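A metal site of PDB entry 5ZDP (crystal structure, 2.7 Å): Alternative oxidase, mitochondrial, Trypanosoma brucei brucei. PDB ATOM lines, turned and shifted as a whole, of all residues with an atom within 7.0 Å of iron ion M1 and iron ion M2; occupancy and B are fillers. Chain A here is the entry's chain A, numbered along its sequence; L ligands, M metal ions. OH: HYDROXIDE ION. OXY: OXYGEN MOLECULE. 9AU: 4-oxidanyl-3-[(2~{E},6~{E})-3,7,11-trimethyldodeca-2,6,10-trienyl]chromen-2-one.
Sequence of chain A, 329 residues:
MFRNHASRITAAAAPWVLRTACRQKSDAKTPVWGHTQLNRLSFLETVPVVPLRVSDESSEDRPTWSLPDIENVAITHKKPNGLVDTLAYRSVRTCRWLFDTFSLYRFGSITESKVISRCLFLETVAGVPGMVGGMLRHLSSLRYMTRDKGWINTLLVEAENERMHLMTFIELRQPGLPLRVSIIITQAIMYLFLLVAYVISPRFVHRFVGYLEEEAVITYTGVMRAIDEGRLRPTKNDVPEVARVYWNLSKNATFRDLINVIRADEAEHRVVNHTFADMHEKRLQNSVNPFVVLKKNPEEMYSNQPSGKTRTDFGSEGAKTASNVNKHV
OE1 of Glu 162 lies close to ND1 of His 165 (2.8 Å). OD1 of Asn 161 lies close to NE2 of His 269 (3.3 Å). OE1 of Glu 123 lies close to ND1 of His 165 (3.3 Å). The side-chain carboxylate (OE1) of Glu 266 sits close to a ring nitrogen (ND1) of His 165, at 3.1 Å. OE1 of Glu 123 lies close to OH of Tyr 220 (3.0 Å). A ring nitrogen (NE2) of His 165 sits at hydrogen-bond distance from the side-chain carboxylate of Asp 265, at 3.3 Å. NE2 of His 269 sits close to O of Asp 265. A ring nitrogen (NE2) of His 165 is in hydrogen-bond range of the side-chain amide oxygen (OD1) of Asn 161 (3.2 Å).
Residues that only touch iron ion M1: His 269. Four residues have an atom within 4 Å of iron ion M1: Glu 162, Glu 213, Glu 266 and His 269. The nearest printed residue that does not touch iron ion M1 is Ala 126 (4.02 Å).
The nearest printed residue that does not touch iron ion M2 is Tyr 220 (4.4 Å).
Iron ion M1 is bound by OE2 of Glu 162 (1.8 Å). Iron ion M1 is bound by the side-chain carboxylate (OE2) of Glu 266, 2.2 Å away. The side-chain carboxylate (OE2) of Glu 213 binds iron ion M1. O of OH L1 is bound to iron ion M1 (2.5 Å). The side-chain carboxylate (OE1) of Glu 213 is bound to iron ion M1. Iron ion M1 has five donor atoms within binding distance.
Iron ion M2 is bound by OE1 of Glu 123 (1.8 Å). The side-chain carboxylate (OE1) of Glu 266 is bound to iron ion M2, 1.8 Å away. Iron ion M2 is bound by OE1 of Glu 162 (2.0 Å). An oxygen (O) of OH L1 is bound to iron ion M2, at 2.2 Å. OE2 of Glu 123 is bound to iron ion M2 (2.3 Å). Iron ion M2 has five donor atoms within binding distance. Slightly farther from iron ion M2 lies ND1 of His 165 (2.7 Å).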
ATOM      1  N   CYS A 119      32.362 -29.168  23.109  1.00  0.00           N
ATOM      2  CA  CYS A 119      31.965 -27.769  23.269  1.00  0.00           C
ATOM      3  C   CYS A 119      30.731 -27.389  22.443  1.00  0.00           C
ATOM      4  O   CYS A 119      29.961 -26.495  22.814  1.00  0.00           O
ATOM      5  CB  CYS A 119      33.153 -26.866  22.889  1.00  0.00           C
ATOM      6  SG  CYS A 119      34.690 -27.336  23.700  1.00  0.00           S
ATOM      7  N   LEU A 122      28.082 -28.927  24.982  1.00  0.00           N
ATOM      8  CA  LEU A 122      28.015 -28.207  26.249  1.00  0.00           C
ATOM      9  C   LEU A 122      27.552 -26.759  26.114  1.00  0.00           C
ATOM     10  O   LEU A 122      27.024 -26.189  27.064  1.00  0.00           O
ATOM     11  CB  LEU A 122      29.359 -28.294  26.975  1.00  0.00           C
ATOM     12  CG  LEU A 122      29.689 -29.697  27.511  1.00  0.00           C
ATOM     13  CD1 LEU A 122      31.090 -29.829  28.089  1.00  0.00           C
ATOM     14  CD2 LEU A 122      28.652 -30.106  28.555  1.00  0.00           C
ATOM     15  N   GLU A 123      27.722 -26.176  24.933  1.00  0.00           N
ATOM     16  CA  GLU A 123      27.248 -24.808  24.676  1.00  0.00           C
ATOM     17  C   GLU A 123      25.770 -24.737  24.329  1.00  0.00           C
ATOM     18  O   GLU A 123      25.164 -23.659  24.408  1.00  0.00           O
ATOM     19  CB  GLU A 123      28.060 -24.130  23.559  1.00  0.00           C
ATOM     20  CG  GLU A 123      29.517 -23.847  23.938  1.00  0.00           C
ATOM     21  CD  GLU A 123      29.696 -22.831  25.062  1.00  0.00           C
ATOM     22  OE1 GLU A 123      30.840 -22.635  25.524  1.00  0.00           O
ATOM     23  OE2 GLU A 123      28.698 -22.207  25.474  1.00  0.00           O
ATOM     24  N   ALA A 126      24.572 -24.204  27.841  1.00  0.00           N
ATOM     25  CA  ALA A 126      25.055 -22.950  28.403  1.00  0.00           C
ATOM     26  C   ALA A 126      24.163 -21.787  28.033  1.00  0.00           C
ATOM     27  O   ALA A 126      23.943 -20.856  28.808  1.00  0.00           O
ATOM     28  CB  ALA A 126      26.477 -22.677  27.923  1.00  0.00           C
ATOM     29  N   GLY A 127      23.617 -21.838  26.832  1.00  0.00           N
ATOM     30  CA  GLY A 127      22.688 -20.819  26.380  1.00  0.00           C
ATOM     31  C   GLY A 127      21.319 -20.875  27.014  1.00  0.00           C
ATOM     32  O   GLY A 127      20.527 -19.957  26.783  1.00  0.00           O
ATOM     33  N   GLU A 158      24.585 -12.660  28.243  1.00  0.00           N
ATOM     34  CA  GLU A 158      25.327 -13.853  28.586  1.00  0.00           C
ATOM     35  C   GLU A 158      24.768 -14.998  27.740  1.00  0.00           C
ATOM     36  O   GLU A 158      25.508 -15.674  27.031  1.00  0.00           O
ATOM     37  CB  GLU A 158      25.208 -14.137  30.091  1.00  0.00           C
ATOM     38  CG  GLU A 158      25.737 -15.499  30.525  1.00  0.00           C
ATOM     39  CD  GLU A 158      25.942 -15.587  32.027  1.00  0.00           C
ATOM     40  OE1 GLU A 158      26.675 -14.716  32.596  1.00  0.00           O
ATOM     41  OE2 GLU A 158      25.369 -16.548  32.633  1.00  0.00           O
ATOM     42  N   ASN A 161      25.767 -14.514  24.301  1.00  0.00           N
ATOM     43  CA  ASN A 161      27.179 -14.804  24.185  1.00  0.00           C
ATOM     44  C   ASN A 161      27.351 -16.308  24.119  1.00  0.00           C
ATOM     45  O   ASN A 161      28.062 -16.812  23.255  1.00  0.00           O
ATOM     46  CB  ASN A 161      27.961 -14.252  25.377  1.00  0.00           C
ATOM     47  CG  ASN A 161      29.412 -14.738  25.402  1.00  0.00           C
ATOM     48  OD1 ASN A 161      29.808 -15.593  26.210  1.00  0.00           O
ATOM     49  ND2 ASN A 161      30.212 -14.196  24.489  1.00  0.00           N
ATOM     50  N   GLU A 162      26.721 -17.041  25.029  1.00  0.00           N
ATOM     51  CA  GLU A 162      26.938 -18.472  25.075  1.00  0.00           C
ATOM     52  C   GLU A 162      26.495 -19.108  23.750  1.00  0.00           C
ATOM     53  O   GLU A 162      27.106 -20.064  23.278  1.00  0.00           O
ATOM     54  CB  GLU A 162      26.264 -19.158  26.280  1.00  0.00           C
ATOM     55  CG  GLU A 162      26.899 -18.889  27.641  1.00  0.00           C
ATOM     56  CD  GLU A 162      28.283 -19.536  27.855  1.00  0.00           C
ATOM     57  OE1 GLU A 162      28.962 -19.905  26.862  1.00  0.00           O
ATOM     58  OE2 GLU A 162      28.715 -19.649  29.032  1.00  0.00           O
ATOM     59  N   ARG A 163      25.450 -18.557  23.134  1.00  0.00           N
ATOM     60  CA  ARG A 163      24.956 -19.074  21.858  1.00  0.00           C
ATOM     61  C   ARG A 163      25.866 -18.653  20.668  1.00  0.00           C
ATOM     62  O   ARG A 163      25.851 -19.297  19.603  1.00  0.00           O
ATOM     63  CB  ARG A 163      23.510 -18.622  21.665  1.00  0.00           C
ATOM     64  CG  ARG A 163      22.724 -19.335  20.571  1.00  0.00           C
ATOM     65  CD  ARG A 163      21.393 -18.630  20.323  1.00  0.00           C
ATOM     66  NE  ARG A 163      21.587 -17.219  19.972  1.00  0.00           N
ATOM     67  CZ  ARG A 163      21.692 -16.730  18.728  1.00  0.00           C
ATOM     68  NH1 ARG A 163      21.878 -15.417  18.555  1.00  0.00           N
ATOM     69  NH2 ARG A 163      21.641 -17.531  17.665  1.00  0.00           N
ATOM     70  N   HIS A 165      29.099 -18.748  21.022  1.00  0.00           N
ATOM     71  CA  HIS A 165      30.040 -19.832  21.162  1.00  0.00           C
ATOM     72  C   HIS A 165      29.591 -21.029  20.339  1.00  0.00           C
ATOM     73  O   HIS A 165      30.411 -21.684  19.709  1.00  0.00           O
ATOM     74  CB  HIS A 165      30.149 -20.246  22.607  1.00  0.00           C
ATOM     75  CG  HIS A 165      30.738 -19.202  23.486  1.00  0.00           C
ATOM     76  ND1 HIS A 165      30.878 -19.359  24.846  1.00  0.00           N
ATOM     77  CD2 HIS A 165      31.244 -17.986  23.198  1.00  0.00           C
ATOM     78  CE1 HIS A 165      31.451 -18.289  25.352  1.00  0.00           C
ATOM     79  NE2 HIS A 165      31.691 -17.441  24.371  1.00  0.00           N
ATOM     80  N   LEU A 166      28.286 -21.320  20.355  1.00  0.00           N
ATOM     81  CA  LEU A 166      27.728 -22.443  19.589  1.00  0.00           C
ATOM     82  C   LEU A 166      27.729 -22.126  18.098  1.00  0.00           C
ATOM     83  O   LEU A 166      28.117 -22.978  17.282  1.00  0.00           O
ATOM     84  CB  LEU A 166      26.293 -22.704  20.032  1.00  0.00           C
ATOM     85  CG  LEU A 166      25.676 -24.096  20.071  1.00  0.00           C
ATOM     86  CD1 LEU A 166      24.293 -24.045  19.458  1.00  0.00           C
ATOM     87  CD2 LEU A 166      26.499 -25.164  19.402  1.00  0.00           C
ATOM     88  N   PHE A 169      31.101 -22.794  17.068  1.00  0.00           N
ATOM     89  CA  PHE A 169      31.476 -24.206  16.985  1.00  0.00           C
ATOM     90  C   PHE A 169      30.728 -24.929  15.868  1.00  0.00           C
ATOM     91  O   PHE A 169      31.329 -25.670  15.089  1.00  0.00           O
ATOM     92  CB  PHE A 169      31.257 -24.895  18.323  1.00  0.00           C
ATOM     93  CG  PHE A 169      32.236 -24.484  19.408  1.00  0.00           C
ATOM     94  CD1 PHE A 169      33.611 -24.592  19.201  1.00  0.00           C
ATOM     95  CD2 PHE A 169      31.784 -24.074  20.650  1.00  0.00           C
ATOM     96  CE1 PHE A 169      34.516 -24.242  20.208  1.00  0.00           C
ATOM     97  CE2 PHE A 169      32.667 -23.729  21.658  1.00  0.00           C
ATOM     98  CZ  PHE A 169      34.039 -23.829  21.433  1.00  0.00           C
ATOM     99  N   VAL A 209      25.638 -22.327  37.707  1.00  0.00           N
ATOM    100  CA  VAL A 209      26.323 -21.796  36.519  1.00  0.00           C
ATOM    101  C   VAL A 209      27.735 -21.311  36.877  1.00  0.00           C
ATOM    102  O   VAL A 209      28.716 -21.600  36.177  1.00  0.00           O
ATOM    103  CB  VAL A 209      25.518 -20.647  35.843  1.00  0.00           C
ATOM    104  CG1 VAL A 209      26.360 -19.869  34.866  1.00  0.00           C
ATOM    105  CG2 VAL A 209      24.292 -21.194  35.136  1.00  0.00           C
ATOM    106  N   LEU A 212      29.736 -24.318  36.918  1.00  0.00           N
ATOM    107  CA  LEU A 212      29.926 -24.870  35.572  1.00  0.00           C
ATOM    108  C   LEU A 212      31.017 -24.103  34.860  1.00  0.00           C
ATOM    109  O   LEU A 212      31.801 -24.678  34.130  1.00  0.00           O
ATOM    110  CB  LEU A 212      28.662 -24.770  34.737  1.00  0.00           C
ATOM    111  CG  LEU A 212      27.556 -25.768  35.031  1.00  0.00           C
ATOM    112  CD1 LEU A 212      26.323 -25.437  34.189  1.00  0.00           C
ATOM    113  CD2 LEU A 212      28.020 -27.210  34.780  1.00  0.00           C
ATOM    114  N   GLU A 213      31.052 -22.787  35.079  1.00  0.00           N
ATOM    115  CA  GLU A 213      32.063 -21.942  34.455  1.00  0.00           C
ATOM    116  C   GLU A 213      33.475 -22.212  35.004  1.00  0.00           C
ATOM    117  O   GLU A 213      34.479 -21.989  34.299  1.00  0.00           O
ATOM    118  CB  GLU A 213      31.708 -20.449  34.625  1.00  0.00           C
ATOM    119  CG  GLU A 213      30.381 -20.024  34.032  1.00  0.00           C
ATOM    120  CD  GLU A 213      30.240 -20.292  32.535  1.00  0.00           C
ATOM    121  OE1 GLU A 213      30.929 -21.194  32.000  1.00  0.00           O
ATOM    122  OE2 GLU A 213      29.397 -19.627  31.891  1.00  0.00           O
ATOM    123  N   ALA A 216      34.416 -24.987  32.885  1.00  0.00           N
ATOM    124  CA  ALA A 216      34.591 -24.560  31.494  1.00  0.00           C
ATOM    125  C   ALA A 216      35.874 -23.744  31.304  1.00  0.00           C
ATOM    126  O   ALA A 216      36.459 -23.773  30.222  1.00  0.00           O
ATOM    127  CB  ALA A 216      33.387 -23.773  31.007  1.00  0.00           C
ATOM    128  N   TYR A 220      38.605 -25.278  28.594  1.00  0.00           N
ATOM    129  CA  TYR A 220      39.253 -24.340  27.654  1.00  0.00           C
ATOM    130  C   TYR A 220      40.701 -24.007  28.016  1.00  0.00           C
ATOM    131  O   TYR A 220      41.449 -23.623  27.130  1.00  0.00           O
ATOM    132  CB  TYR A 220      38.464 -23.033  27.460  1.00  0.00           C
ATOM    133  CG  TYR A 220      37.142 -23.209  26.727  1.00  0.00           C
ATOM    134  CD1 TYR A 220      37.087 -23.825  25.478  1.00  0.00           C
ATOM    135  CD2 TYR A 220      35.954 -22.732  27.274  1.00  0.00           C
ATOM    136  CE1 TYR A 220      35.878 -23.984  24.805  1.00  0.00           C
ATOM    137  CE2 TYR A 220      34.738 -22.885  26.606  1.00  0.00           C
ATOM    138  CZ  TYR A 220      34.708 -23.504  25.373  1.00  0.00           C
ATOM    139  OH  TYR A 220      33.507 -23.657  24.703  1.00  0.00           O
ATOM    140  N   ILE A 262      36.844 -17.174  24.076  1.00  0.00           N
ATOM    141  CA  ILE A 262      35.708 -17.916  24.580  1.00  0.00           C
ATOM    142  C   ILE A 262      35.880 -18.147  26.090  1.00  0.00           C
ATOM    143  O   ILE A 262      34.975 -17.874  26.895  1.00  0.00           O
ATOM    144  CB  ILE A 262      35.479 -19.233  23.807  1.00  0.00           C
ATOM    145  CG1 ILE A 262      34.811 -18.910  22.471  1.00  0.00           C
ATOM    146  CG2 ILE A 262      34.581 -20.163  24.596  1.00  0.00           C
ATOM    147  CD1 ILE A 262      34.779 -20.045  21.477  1.00  0.00           C
ATOM    148  N   ASP A 265      35.050 -15.081  28.312  1.00  0.00           N
ATOM    149  CA  ASP A 265      33.620 -14.935  28.479  1.00  0.00           C
ATOM    150  C   ASP A 265      33.082 -15.853  29.585  1.00  0.00           C
ATOM    151  O   ASP A 265      32.257 -15.436  30.398  1.00  0.00           O
ATOM    152  CB  ASP A 265      32.911 -15.239  27.157  1.00  0.00           C
ATOM    153  CG  ASP A 265      33.137 -14.148  26.114  1.00  0.00           C
ATOM    154  OD1 ASP A 265      33.367 -12.972  26.490  1.00  0.00           O
ATOM    155  OD2 ASP A 265      33.060 -14.461  24.904  1.00  0.00           O
ATOM    156  N   GLU A 266      33.575 -17.092  29.633  1.00  0.00           N
ATOM    157  CA  GLU A 266      33.205 -18.045  30.681  1.00  0.00           C
ATOM    158  C   GLU A 266      33.652 -17.587  32.070  1.00  0.00           C
ATOM    159  O   GLU A 266      33.032 -17.954  33.060  1.00  0.00           O
ATOM    160  CB  GLU A 266      33.800 -19.455  30.427  1.00  0.00           C
ATOM    161  CG  GLU A 266      33.571 -20.050  29.044  1.00  0.00           C
ATOM    162  CD  GLU A 266      32.111 -20.189  28.651  1.00  0.00           C
ATOM    163  OE1 GLU A 266      31.853 -20.584  27.494  1.00  0.00           O
ATOM    164  OE2 GLU A 266      31.201 -19.898  29.467  1.00  0.00           O
ATOM    165  N   HIS A 269      31.344 -14.924  33.234  1.00  0.00           N
ATOM    166  CA  HIS A 269      30.129 -15.596  33.639  1.00  0.00           C
ATOM    167  C   HIS A 269      30.310 -16.145  35.046  1.00  0.00           C
ATOM    168  O   HIS A 269      29.461 -15.982  35.909  1.00  0.00           O
ATOM    169  CB  HIS A 269      29.793 -16.728  32.673  1.00  0.00           C
ATOM    170  CG  HIS A 269      29.505 -16.249  31.291  1.00  0.00           C
ATOM    171  ND1 HIS A 269      29.123 -17.100  30.276  1.00  0.00           N
ATOM    172  CD2 HIS A 269      29.543 -15.011  30.757  1.00  0.00           C
ATOM    173  CE1 HIS A 269      28.952 -16.395  29.169  1.00  0.00           C
ATOM    174  NE2 HIS A 269      29.197 -15.122  29.446  1.00  0.00           N
ATOM    175  N   ARG A 270      31.451 -16.797  35.226  1.00  0.00           N
ATOM    176  CA  ARG A 270      31.884 -17.315  36.506  1.00  0.00           C
ATOM    177  C   ARG A 270      31.685 -16.193  37.541  1.00  0.00           C
ATOM    178  O   ARG A 270      30.830 -16.327  38.406  1.00  0.00           O
ATOM    179  CB  ARG A 270      33.343 -17.799  36.382  1.00  0.00           C
ATOM    180  CG  ARG A 270      33.834 -18.721  37.483  1.00  0.00           C
ATOM    181  CD  ARG A 270      35.284 -19.126  37.254  1.00  0.00           C
ATOM    182  NE  ARG A 270      36.170 -17.971  37.011  1.00  0.00           N
ATOM    183  CZ  ARG A 270      37.410 -18.049  36.532  1.00  0.00           C
ATOM    184  NH1 ARG A 270      37.961 -19.223  36.251  1.00  0.00           N
ATOM    185  NH2 ARG A 270      38.116 -16.925  36.336  1.00  0.00           N
HETATM  186  O    OH L   1      29.506 -22.571  28.176  1.00  0.00           O
HETATM  187  O1  OXY L   2      27.135 -22.425  31.150  1.00  0.00           O
HETATM  188  O2  OXY L   2      27.835 -23.325  30.717  1.00  0.00           O
HETATM  189  OAE 9AU L   3      34.090 -29.469  30.831  1.00  0.00           O
HETATM  190  CAY 9AU L   3      33.302 -28.586  30.433  1.00  0.00           C
HETATM  191  OAS 9AU L   3      33.691 -27.810  29.378  1.00  0.00           O
HETATM  192  CAZ 9AU L   3      32.848 -26.843  28.896  1.00  0.00           C
HETATM  193  CBA 9AU L   3      31.599 -26.639  29.490  1.00  0.00           C
HETATM  194  CAM 9AU L   3      30.771 -25.643  29.009  1.00  0.00           C
HETATM  195  CAK 9AU L   3      31.193 -24.870  27.936  1.00  0.00           C
HETATM  196  CAJ 9AU L   3      32.421 -25.080  27.343  1.00  0.00           C
HETATM  197  CAL 9AU L   3      33.268 -26.065  27.814  1.00  0.00           C
HETATM  198  CAW 9AU L   3      31.207 -27.422  30.575  1.00  0.00           C
HETATM  199  OAF 9AU L   3      29.983 -27.210  31.147  1.00  0.00           O
HETATM  200  CAX 9AU L   3      32.069 -28.408  31.044  1.00  0.00           C
HETATM  201  CAP 9AU L   3      31.745 -29.215  32.233  1.00  0.00           C
HETATM  202  CAI 9AU L   3      30.389 -29.152  32.710  1.00  0.00           C
HETATM  203  CAV 9AU L   3      29.801 -30.312  33.006  1.00  0.00           C
HETATM  204  CAD 9AU L   3      30.613 -31.533  33.105  1.00  0.00           C
HETATM  205  CAR 9AU L   3      28.333 -30.472  33.279  1.00  0.00           C
HETATM  206  CAO 9AU L   3      27.733 -30.741  31.877  1.00  0.00           C
HETATM  207  CAH 9AU L   3      26.685 -31.826  31.840  1.00  0.00           C
HETATM  208  CAU 9AU L   3      25.357 -31.584  31.916  1.00  0.00           C
HETATM  209  CAC 9AU L   3      24.799 -30.202  32.105  1.00  0.00           C
HETATM  210  CAQ 9AU L   3      24.399 -32.757  31.886  1.00  0.00           C
HETATM  211  CAN 9AU L   3      23.431 -32.737  30.721  1.00  0.00           C
HETATM  212  CAG 9AU L   3      22.186 -33.511  31.145  1.00  0.00           C
HETATM  213  CAT 9AU L   3      21.597 -34.484  30.407  1.00  0.00           C
HETATM  214  CAB 9AU L   3      20.386 -35.182  30.924  1.00  0.00           C
HETATM  215  CAA 9AU L   3      22.141 -34.901  29.078  1.00  0.00           C
HETATM  216 FE    FE M   1      29.431 -20.977  30.050  1.00  0.00          FE
HETATM  217 FE    FE M   2      30.415 -21.297  26.652  1.00  0.00          FE
